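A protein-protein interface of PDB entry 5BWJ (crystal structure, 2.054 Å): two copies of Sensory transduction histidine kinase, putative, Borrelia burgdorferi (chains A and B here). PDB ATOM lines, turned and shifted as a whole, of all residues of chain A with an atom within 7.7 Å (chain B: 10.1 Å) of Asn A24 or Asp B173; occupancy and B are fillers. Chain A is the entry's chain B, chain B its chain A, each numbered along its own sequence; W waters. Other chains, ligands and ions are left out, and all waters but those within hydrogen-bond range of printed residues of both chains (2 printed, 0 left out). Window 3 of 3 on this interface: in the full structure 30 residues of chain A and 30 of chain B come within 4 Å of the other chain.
The backbone carbonyl oxygen (O) of Lys A22 lies within hydrogen-bond range of the side-chain hydroxyl (OH) of Tyr A164 (2.7 Å).
O of Tyr A21 lies within hydrogen-bond range of N of Glu A29 (2.8 Å).
The backbone carbonyl oxygen (O) of Phe B94 lies within hydrogen-bond range of the backbone NH (N) of Val B175 (2.8 Å).
The side-chain amide nitrogen of Asn A168 sits at hydrogen-bond distance from the backbone carbonyl oxygen of Tyr A164 (2.9 Å).
The backbone NH (N) of Asn B96 sits at hydrogen-bond distance from the backbone carbonyl oxygen (O) of Asp B173 (2.8 Å).
Among the printed residues, pairs that only touch across the chains: Glu A29 with Val B175 (3.1 Å), Tyr A21 with Ile B176 (3.2 Å), Tyr A164 with His B163 (3.3 Å), Asn A168 with His B163 (3.6 Å) and Glu A29 with Leu B174 (3.7 Å).
Positions printed for both chains: 168 and 169.
Of the 8 pairs that touch across the chains among the printed residues, none has its exchanged pair printed and touching as well.
Water W2 lies within hydrogen-bond range of the side-chain carboxylate of Glu A29 and the backbone carbonyl oxygen of Ile B176.
Water W1 lies within hydrogen-bond range of the backbone carbonyl oxygen (O) of Leu B174 (2.7 Å), the side-chain hydroxyl (OH) of Tyr A21 (3.0 Å) and the side-chain carboxylate (OE1) of Glu A29 (3.4 Å).
Of chain A, only Asn A24 comes within 4 Å of Asp B173.
Asn A23 touches none of the printed residues of chain B.
Printed residues of chain B within 4 Å of Tyr A164: His B163 (3.3 Å).
Printed residues of chain A within 4 Å of Ile B176: Tyr A21 (3.2 Å) and Glu A29 (2.6 Å).
Printed residues of chain A within 4 Å of Leu B174: Glu A29 (3.7 Å).
Printed residues of chain B within 4 Å of Tyr A21: Ile B176.
Ala B166 touches none of the printed residues of chain A.
The nearest residue of chain B that does not touch Asn A24 is Ser B171 (6.7 Å).
The nearest printed residue of chain A that does not touch His B163 is Tyr A21 (4.2 Å).
The side-chain carboxylate of Asp B173 lies within hydrogen-bond range of the side-chain amide nitrogen of Asn A24, 2.7 Å away.
The backbone NH of Ile B176 is in hydrogen-bond range of the side-chain carboxylate of Glu A29.
The side-chain amide oxygen (OD1) of Asn B167 sits close to the side-chain amide oxygen (OD1) of Asn A168 (3.0 Å).
Hydrophobic or aromatic side chains of chain A within 4 Å of the printed part of chain B: Tyr A21 and Tyr A164.
Along chain A the printed residues that touch a printed residue of chain B span positions 21 to 168.
Printed residues of chain B that touch a printed residue of chain A: His B163, Asn B167, Asp B173, Leu B174, Val B175 and Ile B176.
Hydrophobic or aromatic side chains of chain B that line the printed part of chain A: His B163, Val B175 and Ile B176.
Among the printed residues, 8 pairs touch across the chains.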
ATOM      1  N   TYR A  21      32.787  21.860 -16.174  1.00  0.00           N
ATOM      2  CA  TYR A  21      32.378  23.250 -16.023  1.00  0.00           C
ATOM      3  C   TYR A  21      31.220  23.364 -15.041  1.00  0.00           C
ATOM      4  O   TYR A  21      30.497  22.396 -14.811  1.00  0.00           O
ATOM      5  CB  TYR A  21      31.985  23.844 -17.377  1.00  0.00           C
ATOM      6  CG  TYR A  21      30.894  23.078 -18.093  1.00  0.00           C
ATOM      7  CD1 TYR A  21      31.194  21.966 -18.871  1.00  0.00           C
ATOM      8  CD2 TYR A  21      29.565  23.469 -17.995  1.00  0.00           C
ATOM      9  CE1 TYR A  21      30.201  21.266 -19.529  1.00  0.00           C
ATOM     10  CE2 TYR A  21      28.566  22.774 -18.650  1.00  0.00           C
ATOM     11  CZ  TYR A  21      28.889  21.673 -19.416  1.00  0.00           C
ATOM     12  OH  TYR A  21      27.897  20.979 -20.069  1.00  0.00           O
ATOM     13  N   LYS A  22      31.048  24.552 -14.467  1.00  0.00           N
ATOM     14  CA  LYS A  22      30.015  24.775 -13.461  1.00  0.00           C
ATOM     15  C   LYS A  22      28.638  24.965 -14.085  1.00  0.00           C
ATOM     16  O   LYS A  22      28.496  25.649 -15.100  1.00  0.00           O
ATOM     17  CB  LYS A  22      30.348  26.002 -12.609  1.00  0.00           C
ATOM     18  CG  LYS A  22      31.637  25.900 -11.817  1.00  0.00           C
ATOM     19  CD  LYS A  22      31.826  27.135 -10.944  1.00  0.00           C
ATOM     20  CE  LYS A  22      33.194  27.162 -10.289  1.00  0.00           C
ATOM     21  NZ  LYS A  22      33.399  28.398  -9.483  1.00  0.00           N
ATOM     22  N   ASN A  23      27.630  24.359 -13.461  1.00  0.00           N
ATOM     23  CA  ASN A  23      26.236  24.580 -13.835  1.00  0.00           C
ATOM     24  C   ASN A  23      25.557  25.527 -12.843  1.00  0.00           C
ATOM     25  O   ASN A  23      26.215  26.092 -11.970  1.00  0.00           O
ATOM     26  CB  ASN A  23      25.483  23.247 -13.915  1.00  0.00           C
ATOM     27  CG  ASN A  23      25.525  22.463 -12.613  1.00  0.00           C
ATOM     28  OD1 ASN A  23      25.808  23.008 -11.544  1.00  0.00           O
ATOM     29  ND2 ASN A  23      25.233  21.170 -12.700  1.00  0.00           N
ATOM     30  N   ASN A  24      24.245  25.697 -12.976  1.00  0.00           N
ATOM     31  CA  ASN A  24      23.497  26.613 -12.117  1.00  0.00           C
ATOM     32  C   ASN A  24      23.372  26.123 -10.677  1.00  0.00           C
ATOM     33  O   ASN A  24      23.090  26.908  -9.772  1.00  0.00           O
ATOM     34  CB  ASN A  24      22.096  26.847 -12.687  1.00  0.00           C
ATOM     35  CG  ASN A  24      22.113  27.644 -13.976  1.00  0.00           C
ATOM     36  OD1 ASN A  24      23.117  28.264 -14.327  1.00  0.00           O
ATOM     37  ND2 ASN A  24      20.990  27.641 -14.685  1.00  0.00           N
ATOM     38  N   LYS A  25      23.580  24.828 -10.469  1.00  0.00           N
ATOM     39  CA  LYS A  25      23.389  24.224  -9.155  1.00  0.00           C
ATOM     40  C   LYS A  25      24.673  24.228  -8.329  1.00  0.00           C
ATOM     41  O   LYS A  25      24.748  23.581  -7.285  1.00  0.00           O
ATOM     42  CB  LYS A  25      22.875  22.793  -9.309  1.00  0.00           C
ATOM     43  CG  LYS A  25      21.653  22.679 -10.214  1.00  0.00           C
ATOM     44  CD  LYS A  25      21.144  21.248 -10.309  1.00  0.00           C
ATOM     45  CE  LYS A  25      22.181  20.319 -10.922  1.00  0.00           C
ATOM     46  NZ  LYS A  25      21.621  18.971 -11.210  1.00  0.00           N
ATOM     47  N   GLY A  26      25.679  24.959  -8.797  1.00  0.00           N
ATOM     48  CA  GLY A  26      26.952  25.030  -8.103  1.00  0.00           C
ATOM     49  C   GLY A  26      27.763  23.751  -8.218  1.00  0.00           C
ATOM     50  O   GLY A  26      28.787  23.600  -7.551  1.00  0.00           O
ATOM     51  N   GLU A  27      27.305  22.834  -9.066  1.00  0.00           N
ATOM     52  CA  GLU A  27      27.987  21.562  -9.274  1.00  0.00           C
ATOM     53  C   GLU A  27      28.785  21.592 -10.572  1.00  0.00           C
ATOM     54  O   GLU A  27      28.655  22.522 -11.369  1.00  0.00           O
ATOM     55  CB  GLU A  27      26.980  20.410  -9.305  1.00  0.00           C
ATOM     56  N   GLU A  29      29.431  19.908 -14.118  1.00  0.00           N
ATOM     57  CA  GLU A  29      28.982  19.052 -15.203  1.00  0.00           C
ATOM     58  C   GLU A  29      30.140  18.829 -16.168  1.00  0.00           C
ATOM     59  O   GLU A  29      31.044  19.657 -16.254  1.00  0.00           O
ATOM     60  CB  GLU A  29      27.790  19.685 -15.920  1.00  0.00           C
ATOM     61  CG  GLU A  29      27.227  18.844 -17.051  1.00  0.00           C
ATOM     62  CD  GLU A  29      25.723  18.707 -16.982  1.00  0.00           C
ATOM     63  OE1 GLU A  29      25.042  19.697 -16.636  1.00  0.00           O
ATOM     64  OE2 GLU A  29      25.222  17.601 -17.266  1.00  0.00           O
ATOM     65  N   TYR A 164      31.106  30.371 -22.676  1.00  0.00           N
ATOM     66  CA  TYR A 164      30.072  29.635 -21.962  1.00  0.00           C
ATOM     67  C   TYR A 164      29.692  30.334 -20.659  1.00  0.00           C
ATOM     68  O   TYR A 164      28.513  30.556 -20.388  1.00  0.00           O
ATOM     69  CB  TYR A 164      30.527  28.207 -21.655  1.00  0.00           C
ATOM     70  CG  TYR A 164      29.699  27.558 -20.567  1.00  0.00           C
ATOM     71  CD1 TYR A 164      28.449  27.022 -20.847  1.00  0.00           C
ATOM     72  CD2 TYR A 164      30.158  27.498 -19.258  1.00  0.00           C
ATOM     73  CE1 TYR A 164      27.680  26.438 -19.855  1.00  0.00           C
ATOM     74  CE2 TYR A 164      29.396  26.914 -18.258  1.00  0.00           C
ATOM     75  CZ  TYR A 164      28.159  26.387 -18.564  1.00  0.00           C
ATOM     76  OH  TYR A 164      27.397  25.803 -17.576  1.00  0.00           O
ATOM     77  N   ASN A 168      26.022  31.951 -19.960  1.00  0.00           N
ATOM     78  CA  ASN A 168      25.126  31.176 -19.106  1.00  0.00           C
ATOM     79  C   ASN A 168      24.969  31.727 -17.686  1.00  0.00           C
ATOM     80  O   ASN A 168      23.939  31.501 -17.048  1.00  0.00           O
ATOM     81  CB  ASN A 168      25.609  29.726 -19.035  1.00  0.00           C
ATOM     82  CG  ASN A 168      25.328  28.955 -20.314  1.00  0.00           C
ATOM     83  OD1 ASN A 168      24.335  28.231 -20.413  1.00  0.00           O
ATOM     84  ND2 ASN A 168      26.200  29.112 -21.305  1.00  0.00           N
ATOM     85  N   PHE A 169      25.983  32.440 -17.194  1.00  0.00           N
ATOM     86  CA  PHE A 169      25.962  32.957 -15.822  1.00  0.00           C
ATOM     87  C   PHE A 169      25.709  34.462 -15.746  1.00  0.00           C
ATOM     88  O   PHE A 169      25.148  34.948 -14.763  1.00  0.00           O
ATOM     89  CB  PHE A 169      27.280  32.641 -15.108  1.00  0.00           C
ATOM     90  CG  PHE A 169      27.440  31.196 -14.737  1.00  0.00           C
ATOM     91  CD1 PHE A 169      26.676  30.642 -13.725  1.00  0.00           C
ATOM     92  CD2 PHE A 169      28.365  30.396 -15.386  1.00  0.00           C
ATOM     93  CE1 PHE A 169      26.821  29.314 -13.374  1.00  0.00           C
ATOM     94  CE2 PHE A 169      28.517  29.066 -15.039  1.00  0.00           C
ATOM     95  CZ  PHE A 169      27.743  28.525 -14.029  1.00  0.00           C
ATOM     96  N   LEU B  92      25.316  13.940 -25.907  1.00  0.00           N
ATOM     97  CA  LEU B  92      23.879  13.741 -25.828  1.00  0.00           C
ATOM     98  C   LEU B  92      23.316  14.625 -24.714  1.00  0.00           C
ATOM     99  O   LEU B  92      23.669  14.457 -23.543  1.00  0.00           O
ATOM    100  CB  LEU B  92      23.558  12.268 -25.571  1.00  0.00           C
ATOM    101  CG  LEU B  92      22.089  11.862 -25.684  1.00  0.00           C
ATOM    102  CD1 LEU B  92      21.663  11.801 -27.140  1.00  0.00           C
ATOM    103  CD2 LEU B  92      21.852  10.530 -24.997  1.00  0.00           C
ATOM    104  N   PHE B  93      22.457  15.571 -25.087  1.00  0.00           N
ATOM    105  CA  PHE B  93      21.862  16.515 -24.140  1.00  0.00           C
ATOM    106  C   PHE B  93      20.396  16.199 -23.868  1.00  0.00           C
ATOM    107  O   PHE B  93      19.699  15.676 -24.735  1.00  0.00           O
ATOM    108  CB  PHE B  93      21.955  17.950 -24.668  1.00  0.00           C
ATOM    109  CG  PHE B  93      23.354  18.492 -24.752  1.00  0.00           C
ATOM    110  CD1 PHE B  93      24.043  18.858 -23.607  1.00  0.00           C
ATOM    111  CD2 PHE B  93      23.965  18.674 -25.981  1.00  0.00           C
ATOM    112  CE1 PHE B  93      25.323  19.372 -23.685  1.00  0.00           C
ATOM    113  CE2 PHE B  93      25.246  19.189 -26.066  1.00  0.00           C
ATOM    114  CZ  PHE B  93      25.924  19.539 -24.919  1.00  0.00           C
ATOM    115  N   PHE B  94      19.934  16.532 -22.666  1.00  0.00           N
ATOM    116  CA  PHE B  94      18.506  16.567 -22.371  1.00  0.00           C
ATOM    117  C   PHE B  94      18.219  17.750 -21.453  1.00  0.00           C
ATOM    118  O   PHE B  94      19.139  18.347 -20.895  1.00  0.00           O
ATOM    119  CB  PHE B  94      18.030  15.251 -21.744  1.00  0.00           C
ATOM    120  CG  PHE B  94      18.760  14.868 -20.489  1.00  0.00           C
ATOM    121  CD1 PHE B  94      18.238  15.183 -19.245  1.00  0.00           C
ATOM    122  CD2 PHE B  94      19.960  14.176 -20.552  1.00  0.00           C
ATOM    123  CE1 PHE B  94      18.904  14.826 -18.087  1.00  0.00           C
ATOM    124  CE2 PHE B  94      20.631  13.816 -19.398  1.00  0.00           C
ATOM    125  CZ  PHE B  94      20.102  14.142 -18.164  1.00  0.00           C
ATOM    126  N   LYS B  95      16.944  18.100 -21.313  1.00  0.00           N
ATOM    127  CA  LYS B  95      16.556  19.252 -20.507  1.00  0.00           C
ATOM    128  C   LYS B  95      16.561  18.919 -19.023  1.00  0.00           C
ATOM    129  O   LYS B  95      16.182  17.821 -18.622  1.00  0.00           O
ATOM    130  CB  LYS B  95      15.171  19.756 -20.917  1.00  0.00           C
ATOM    131  CG  LYS B  95      15.125  20.342 -22.317  1.00  0.00           C
ATOM    132  CD  LYS B  95      13.805  21.043 -22.594  1.00  0.00           C
ATOM    133  CE  LYS B  95      12.634  20.076 -22.566  1.00  0.00           C
ATOM    134  NZ  LYS B  95      11.364  20.734 -22.986  1.00  0.00           N
ATOM    135  N   ASN B  96      16.999  19.879 -18.217  1.00  0.00           N
ATOM    136  CA  ASN B  96      16.973  19.737 -16.768  1.00  0.00           C
ATOM    137  C   ASN B  96      15.556  19.877 -16.220  1.00  0.00           C
ATOM    138  O   ASN B  96      14.944  18.896 -15.796  1.00  0.00           O
ATOM    139  CB  ASN B  96      17.887  20.777 -16.118  1.00  0.00           C
ATOM    140  CG  ASN B  96      17.845  20.727 -14.607  1.00  0.00           C
ATOM    141  OD1 ASN B  96      17.189  21.548 -13.965  1.00  0.00           O
ATOM    142  ND2 ASN B  96      18.543  19.757 -14.028  1.00  0.00           N
ATOM    143  N   LEU B 147      13.661  19.674 -29.135  1.00  0.00           N
ATOM    144  CA  LEU B 147      13.851  19.398 -27.716  1.00  0.00           C
ATOM    145  C   LEU B 147      12.963  20.305 -26.872  1.00  0.00           C
ATOM    146  O   LEU B 147      12.386  19.868 -25.879  1.00  0.00           O
ATOM    147  CB  LEU B 147      15.318  19.583 -27.320  1.00  0.00           C
ATOM    148  CG  LEU B 147      15.668  19.235 -25.871  1.00  0.00           C
ATOM    149  CD1 LEU B 147      15.441  17.756 -25.590  1.00  0.00           C
ATOM    150  CD2 LEU B 147      17.104  19.621 -25.569  1.00  0.00           C
ATOM    151  N   LYS B 148      12.862  21.569 -27.276  1.00  0.00           N
ATOM    152  CA  LYS B 148      12.043  22.545 -26.562  1.00  0.00           C
ATOM    153  C   LYS B 148      10.596  22.092 -26.461  1.00  0.00           C
ATOM    154  O   LYS B 148      10.004  22.106 -25.384  1.00  0.00           O
ATOM    155  CB  LYS B 148      12.081  23.907 -27.258  1.00  0.00           C
ATOM    156  CG  LYS B 148      11.471  25.021 -26.414  1.00  0.00           C
ATOM    157  CD  LYS B 148      11.551  26.372 -27.093  1.00  0.00           C
ATOM    158  CE  LYS B 148      10.923  27.456 -26.229  1.00  0.00           C
ATOM    159  NZ  LYS B 148      10.995  28.797 -26.871  1.00  0.00           N
ATOM    160  N   ASP B 153      13.342  13.591 -26.547  1.00  0.00           N
ATOM    161  CA  ASP B 153      13.784  13.597 -25.155  1.00  0.00           C
ATOM    162  C   ASP B 153      15.261  13.961 -25.048  1.00  0.00           C
ATOM    163  O   ASP B 153      15.693  14.558 -24.060  1.00  0.00           O
ATOM    164  CB  ASP B 153      13.534  12.234 -24.516  1.00  0.00           C
ATOM    165  CG  ASP B 153      12.078  11.820 -24.585  1.00  0.00           C
ATOM    166  OD1 ASP B 153      11.256  12.421 -23.863  1.00  0.00           O
ATOM    167  OD2 ASP B 153      11.757  10.894 -25.357  1.00  0.00           O
ATOM    168  N   ILE B 155      18.895  15.278 -27.517  1.00  0.00           N
ATOM    169  CA  ILE B 155      19.512  15.683 -28.773  1.00  0.00           C
ATOM    170  C   ILE B 155      20.985  15.281 -28.755  1.00  0.00           C
ATOM    171  O   ILE B 155      21.634  15.303 -27.707  1.00  0.00           O
ATOM    172  CB  ILE B 155      19.371  17.201 -29.039  1.00  0.00           C
ATOM    173  CG1 ILE B 155      20.025  18.024 -27.925  1.00  0.00           C
ATOM    174  CG2 ILE B 155      17.899  17.567 -29.192  1.00  0.00           C
ATOM    175  CD1 ILE B 155      20.109  19.510 -28.230  1.00  0.00           C
ATOM    176  N   LEU B 162      25.461  23.162 -30.254  1.00  0.00           N
ATOM    177  CA  LEU B 162      24.117  22.814 -29.799  1.00  0.00           C
ATOM    178  C   LEU B 162      23.822  23.412 -28.433  1.00  0.00           C
ATOM    179  O   LEU B 162      22.712  23.882 -28.184  1.00  0.00           O
ATOM    180  CB  LEU B 162      23.924  21.298 -29.737  1.00  0.00           C
ATOM    181  CG  LEU B 162      23.637  20.564 -31.047  1.00  0.00           C
ATOM    182  CD1 LEU B 162      23.370  19.096 -30.751  1.00  0.00           C
ATOM    183  CD2 LEU B 162      22.462  21.175 -31.802  1.00  0.00           C
ATOM    184  N   HIS B 163      24.809  23.387 -27.546  1.00  0.00           N
ATOM    185  CA  HIS B 163      24.629  23.944 -26.214  1.00  0.00           C
ATOM    186  C   HIS B 163      24.338  25.432 -26.329  1.00  0.00           C
ATOM    187  O   HIS B 163      23.461  25.962 -25.652  1.00  0.00           O
ATOM    188  CB  HIS B 163      25.867  23.708 -25.346  1.00  0.00           C
ATOM    189  CG  HIS B 163      25.695  24.140 -23.925  1.00  0.00           C
ATOM    190  ND1 HIS B 163      25.442  23.253 -22.902  1.00  0.00           N
ATOM    191  CD2 HIS B 163      25.729  25.370 -23.357  1.00  0.00           C
ATOM    192  CE1 HIS B 163      25.334  23.915 -21.763  1.00  0.00           C
ATOM    193  NE2 HIS B 163      25.502  25.201 -22.013  1.00  0.00           N
ATOM    194  N   ALA B 166      20.895  26.095 -27.879  1.00  0.00           N
ATOM    195  CA  ALA B 166      19.918  25.672 -26.881  1.00  0.00           C
ATOM    196  C   ALA B 166      19.678  26.765 -25.844  1.00  0.00           C
ATOM    197  O   ALA B 166      18.534  27.054 -25.484  1.00  0.00           O
ATOM    198  CB  ALA B 166      20.375  24.391 -26.202  1.00  0.00           C
ATOM    199  N   ASN B 167      20.757  27.379 -25.371  1.00  0.00           N
ATOM    200  CA  ASN B 167      20.654  28.419 -24.355  1.00  0.00           C
ATOM    201  C   ASN B 167      19.971  29.676 -24.892  1.00  0.00           C
ATOM    202  O   ASN B 167      19.534  30.531 -24.122  1.00  0.00           O
ATOM    203  CB  ASN B 167      22.041  28.768 -23.813  1.00  0.00           C
ATOM    204  CG  ASN B 167      21.980  29.640 -22.574  1.00  0.00           C
ATOM    205  OD1 ASN B 167      21.718  29.154 -21.473  1.00  0.00           O
ATOM    206  ND2 ASN B 167      22.227  30.934 -22.748  1.00  0.00           N
ATOM    207  N   ASN B 168      19.881  29.778 -26.216  1.00  0.00           N
ATOM    208  CA  ASN B 168      19.249  30.924 -26.861  1.00  0.00           C
ATOM    209  C   ASN B 168      17.743  30.742 -27.039  1.00  0.00           C
ATOM    210  O   ASN B 168      17.012  31.722 -27.187  1.00  0.00           O
ATOM    211  CB  ASN B 168      19.894  31.181 -28.224  1.00  0.00           C
ATOM    212  CG  ASN B 168      21.367  31.531 -28.118  1.00  0.00           C
ATOM    213  OD1 ASN B 168      21.959  31.466 -27.037  1.00  0.00           O
ATOM    214  ND2 ASN B 168      21.968  31.903 -29.243  1.00  0.00           N
ATOM    215  N   PHE B 169      17.285  29.492 -27.023  1.00  0.00           N
ATOM    216  CA  PHE B 169      15.876  29.184 -27.265  1.00  0.00           C
ATOM    217  C   PHE B 169      15.187  28.517 -26.074  1.00  0.00           C
ATOM    218  O   PHE B 169      13.972  28.635 -25.920  1.00  0.00           O
ATOM    219  CB  PHE B 169      15.742  28.286 -28.498  1.00  0.00           C
ATOM    220  CG  PHE B 169      16.002  28.995 -29.794  1.00  0.00           C
ATOM    221  CD1 PHE B 169      15.025  29.790 -30.373  1.00  0.00           C
ATOM    222  CD2 PHE B 169      17.221  28.867 -30.438  1.00  0.00           C
ATOM    223  CE1 PHE B 169      15.261  30.446 -31.567  1.00  0.00           C
ATOM    224  CE2 PHE B 169      17.462  29.519 -31.632  1.00  0.00           C
ATOM    225  CZ  PHE B 169      16.480  30.309 -32.198  1.00  0.00           C
ATOM    226  N   LEU B 170      15.952  27.817 -25.241  1.00  0.00           N
ATOM    227  CA  LEU B 170      15.373  27.080 -24.117  1.00  0.00           C
ATOM    228  C   LEU B 170      15.435  27.869 -22.814  1.00  0.00           C
ATOM    229  O   LEU B 170      16.374  28.630 -22.579  1.00  0.00           O
ATOM    230  CB  LEU B 170      16.087  25.739 -23.927  1.00  0.00           C
ATOM    231  CG  LEU B 170      16.187  24.796 -25.132  1.00  0.00           C
ATOM    232  CD1 LEU B 170      16.429  23.372 -24.659  1.00  0.00           C
ATOM    233  CD2 LEU B 170      14.954  24.853 -25.997  1.00  0.00           C
ATOM    234  N   SER B 171      14.427  27.671 -21.971  1.00  0.00           N
ATOM    235  CA  SER B 171      14.397  28.270 -20.641  1.00  0.00           C
ATOM    236  C   SER B 171      15.036  27.327 -19.625  1.00  0.00           C
ATOM    237  O   SER B 171      15.541  27.763 -18.591  1.00  0.00           O
ATOM    238  CB  SER B 171      12.960  28.602 -20.229  1.00  0.00           C
ATOM    239  OG  SER B 171      12.158  27.435 -20.183  1.00  0.00           O
ATOM    240  N   GLU B 172      15.010  26.032 -19.931  1.00  0.00           N
ATOM    241  CA  GLU B 172      15.622  25.022 -19.073  1.00  0.00           C
ATOM    242  C   GLU B 172      17.089  24.825 -19.434  1.00  0.00           C
ATOM    243  O   GLU B 172      17.483  25.002 -20.588  1.00  0.00           O
ATOM    244  CB  GLU B 172      14.872  23.693 -19.191  1.00  0.00           C
ATOM    245  CG  GLU B 172      13.416  23.754 -18.748  1.00  0.00           C
ATOM    246  CD  GLU B 172      13.261  24.007 -17.259  1.00  0.00           C
ATOM    247  OE1 GLU B 172      14.187  23.666 -16.492  1.00  0.00           O
ATOM    248  OE2 GLU B 172      12.210  24.549 -16.855  1.00  0.00           O
ATOM    249  N   ASP B 173      17.895  24.458 -18.445  1.00  0.00           N
ATOM    250  CA  ASP B 173      19.306  24.181 -18.677  1.00  0.00           C
ATOM    251  C   ASP B 173      19.480  22.812 -19.321  1.00  0.00           C
ATOM    252  O   ASP B 173      18.692  21.895 -19.078  1.00  0.00           O
ATOM    253  CB  ASP B 173      20.095  24.246 -17.366  1.00  0.00           C
ATOM    254  CG  ASP B 173      20.017  25.606 -16.705  1.00  0.00           C
ATOM    255  OD1 ASP B 173      20.725  26.530 -17.159  1.00  0.00           O
ATOM    256  OD2 ASP B 173      19.254  25.751 -15.727  1.00  0.00           O
ATOM    257  N   LEU B 174      20.511  22.685 -20.148  1.00  0.00           N
ATOM    258  CA  LEU B 174      20.883  21.401 -20.724  1.00  0.00           C
ATOM    259  C   LEU B 174      21.717  20.587 -19.746  1.00  0.00           C
ATOM    260  O   LEU B 174      22.545  21.134 -19.018  1.00  0.00           O
ATOM    261  CB  LEU B 174      21.666  21.598 -22.022  1.00  0.00           C
ATOM    262  CG  LEU B 174      20.849  21.546 -23.312  1.00  0.00           C
ATOM    263  CD1 LEU B 174      19.662  22.484 -23.247  1.00  0.00           C
ATOM    264  CD2 LEU B 174      21.731  21.880 -24.504  1.00  0.00           C
ATOM    265  N   VAL B 175      21.494  19.278 -19.747  1.00  0.00           N
ATOM    266  CA  VAL B 175      22.273  18.352 -18.935  1.00  0.00           C
ATOM    267  C   VAL B 175      22.944  17.339 -19.858  1.00  0.00           C
ATOM    268  O   VAL B 175      22.362  16.928 -20.860  1.00  0.00           O
ATOM    269  CB  VAL B 175      21.392  17.624 -17.897  1.00  0.00           C
ATOM    270  CG1 VAL B 175      22.230  16.701 -17.025  1.00  0.00           C
ATOM    271  CG2 VAL B 175      20.648  18.633 -17.031  1.00  0.00           C
ATOM    272  N   ILE B 176      24.171  16.954 -19.521  1.00  0.00           N
ATOM    273  CA  ILE B 176      24.897  15.946 -20.283  1.00  0.00           C
ATOM    274  C   ILE B 176      24.536  14.545 -19.810  1.00  0.00           C
ATOM    275  O   ILE B 176      24.580  14.248 -18.615  1.00  0.00           O
ATOM    276  CB  ILE B 176      26.425  16.139 -20.170  1.00  0.00           C
ATOM    277  CG1 ILE B 176      26.834  17.470 -20.801  1.00  0.00           C
ATOM    278  CG2 ILE B 176      27.171  14.984 -20.853  1.00  0.00           C
ATOM    279  CD1 ILE B 176      28.302  17.818 -20.621  1.00  0.00           C
ATOM    280  N   PHE B 177      24.180  13.689 -20.761  1.00  0.00           N
ATOM    281  CA  PHE B 177      23.956  12.276 -20.483  1.00  0.00           C
ATOM    282  C   PHE B 177      25.298  11.566 -20.356  1.00  0.00           C
ATOM    283  O   PHE B 177      26.032  11.434 -21.335  1.00  0.00           O
ATOM    284  CB  PHE B 177      23.115  11.637 -21.588  1.00  0.00           C
ATOM    285  CG  PHE B 177      22.922  10.157 -21.428  1.00  0.00           C
ATOM    286  CD1 PHE B 177      23.735   9.262 -22.105  1.00  0.00           C
ATOM    287  CD2 PHE B 177      21.925   9.659 -20.606  1.00  0.00           C
ATOM    288  CE1 PHE B 177      23.559   7.899 -21.964  1.00  0.00           C
ATOM    289  CE2 PHE B 177      21.744   8.297 -20.460  1.00  0.00           C
ATOM    290  CZ  PHE B 177      22.562   7.416 -21.140  1.00  0.00           C
HETATM  291  O   HOH W   1      25.118  21.807 -19.339  1.00  0.00           O
HETATM  292  O   HOH W   2      26.013  15.398 -16.405  1.00  0.00           O
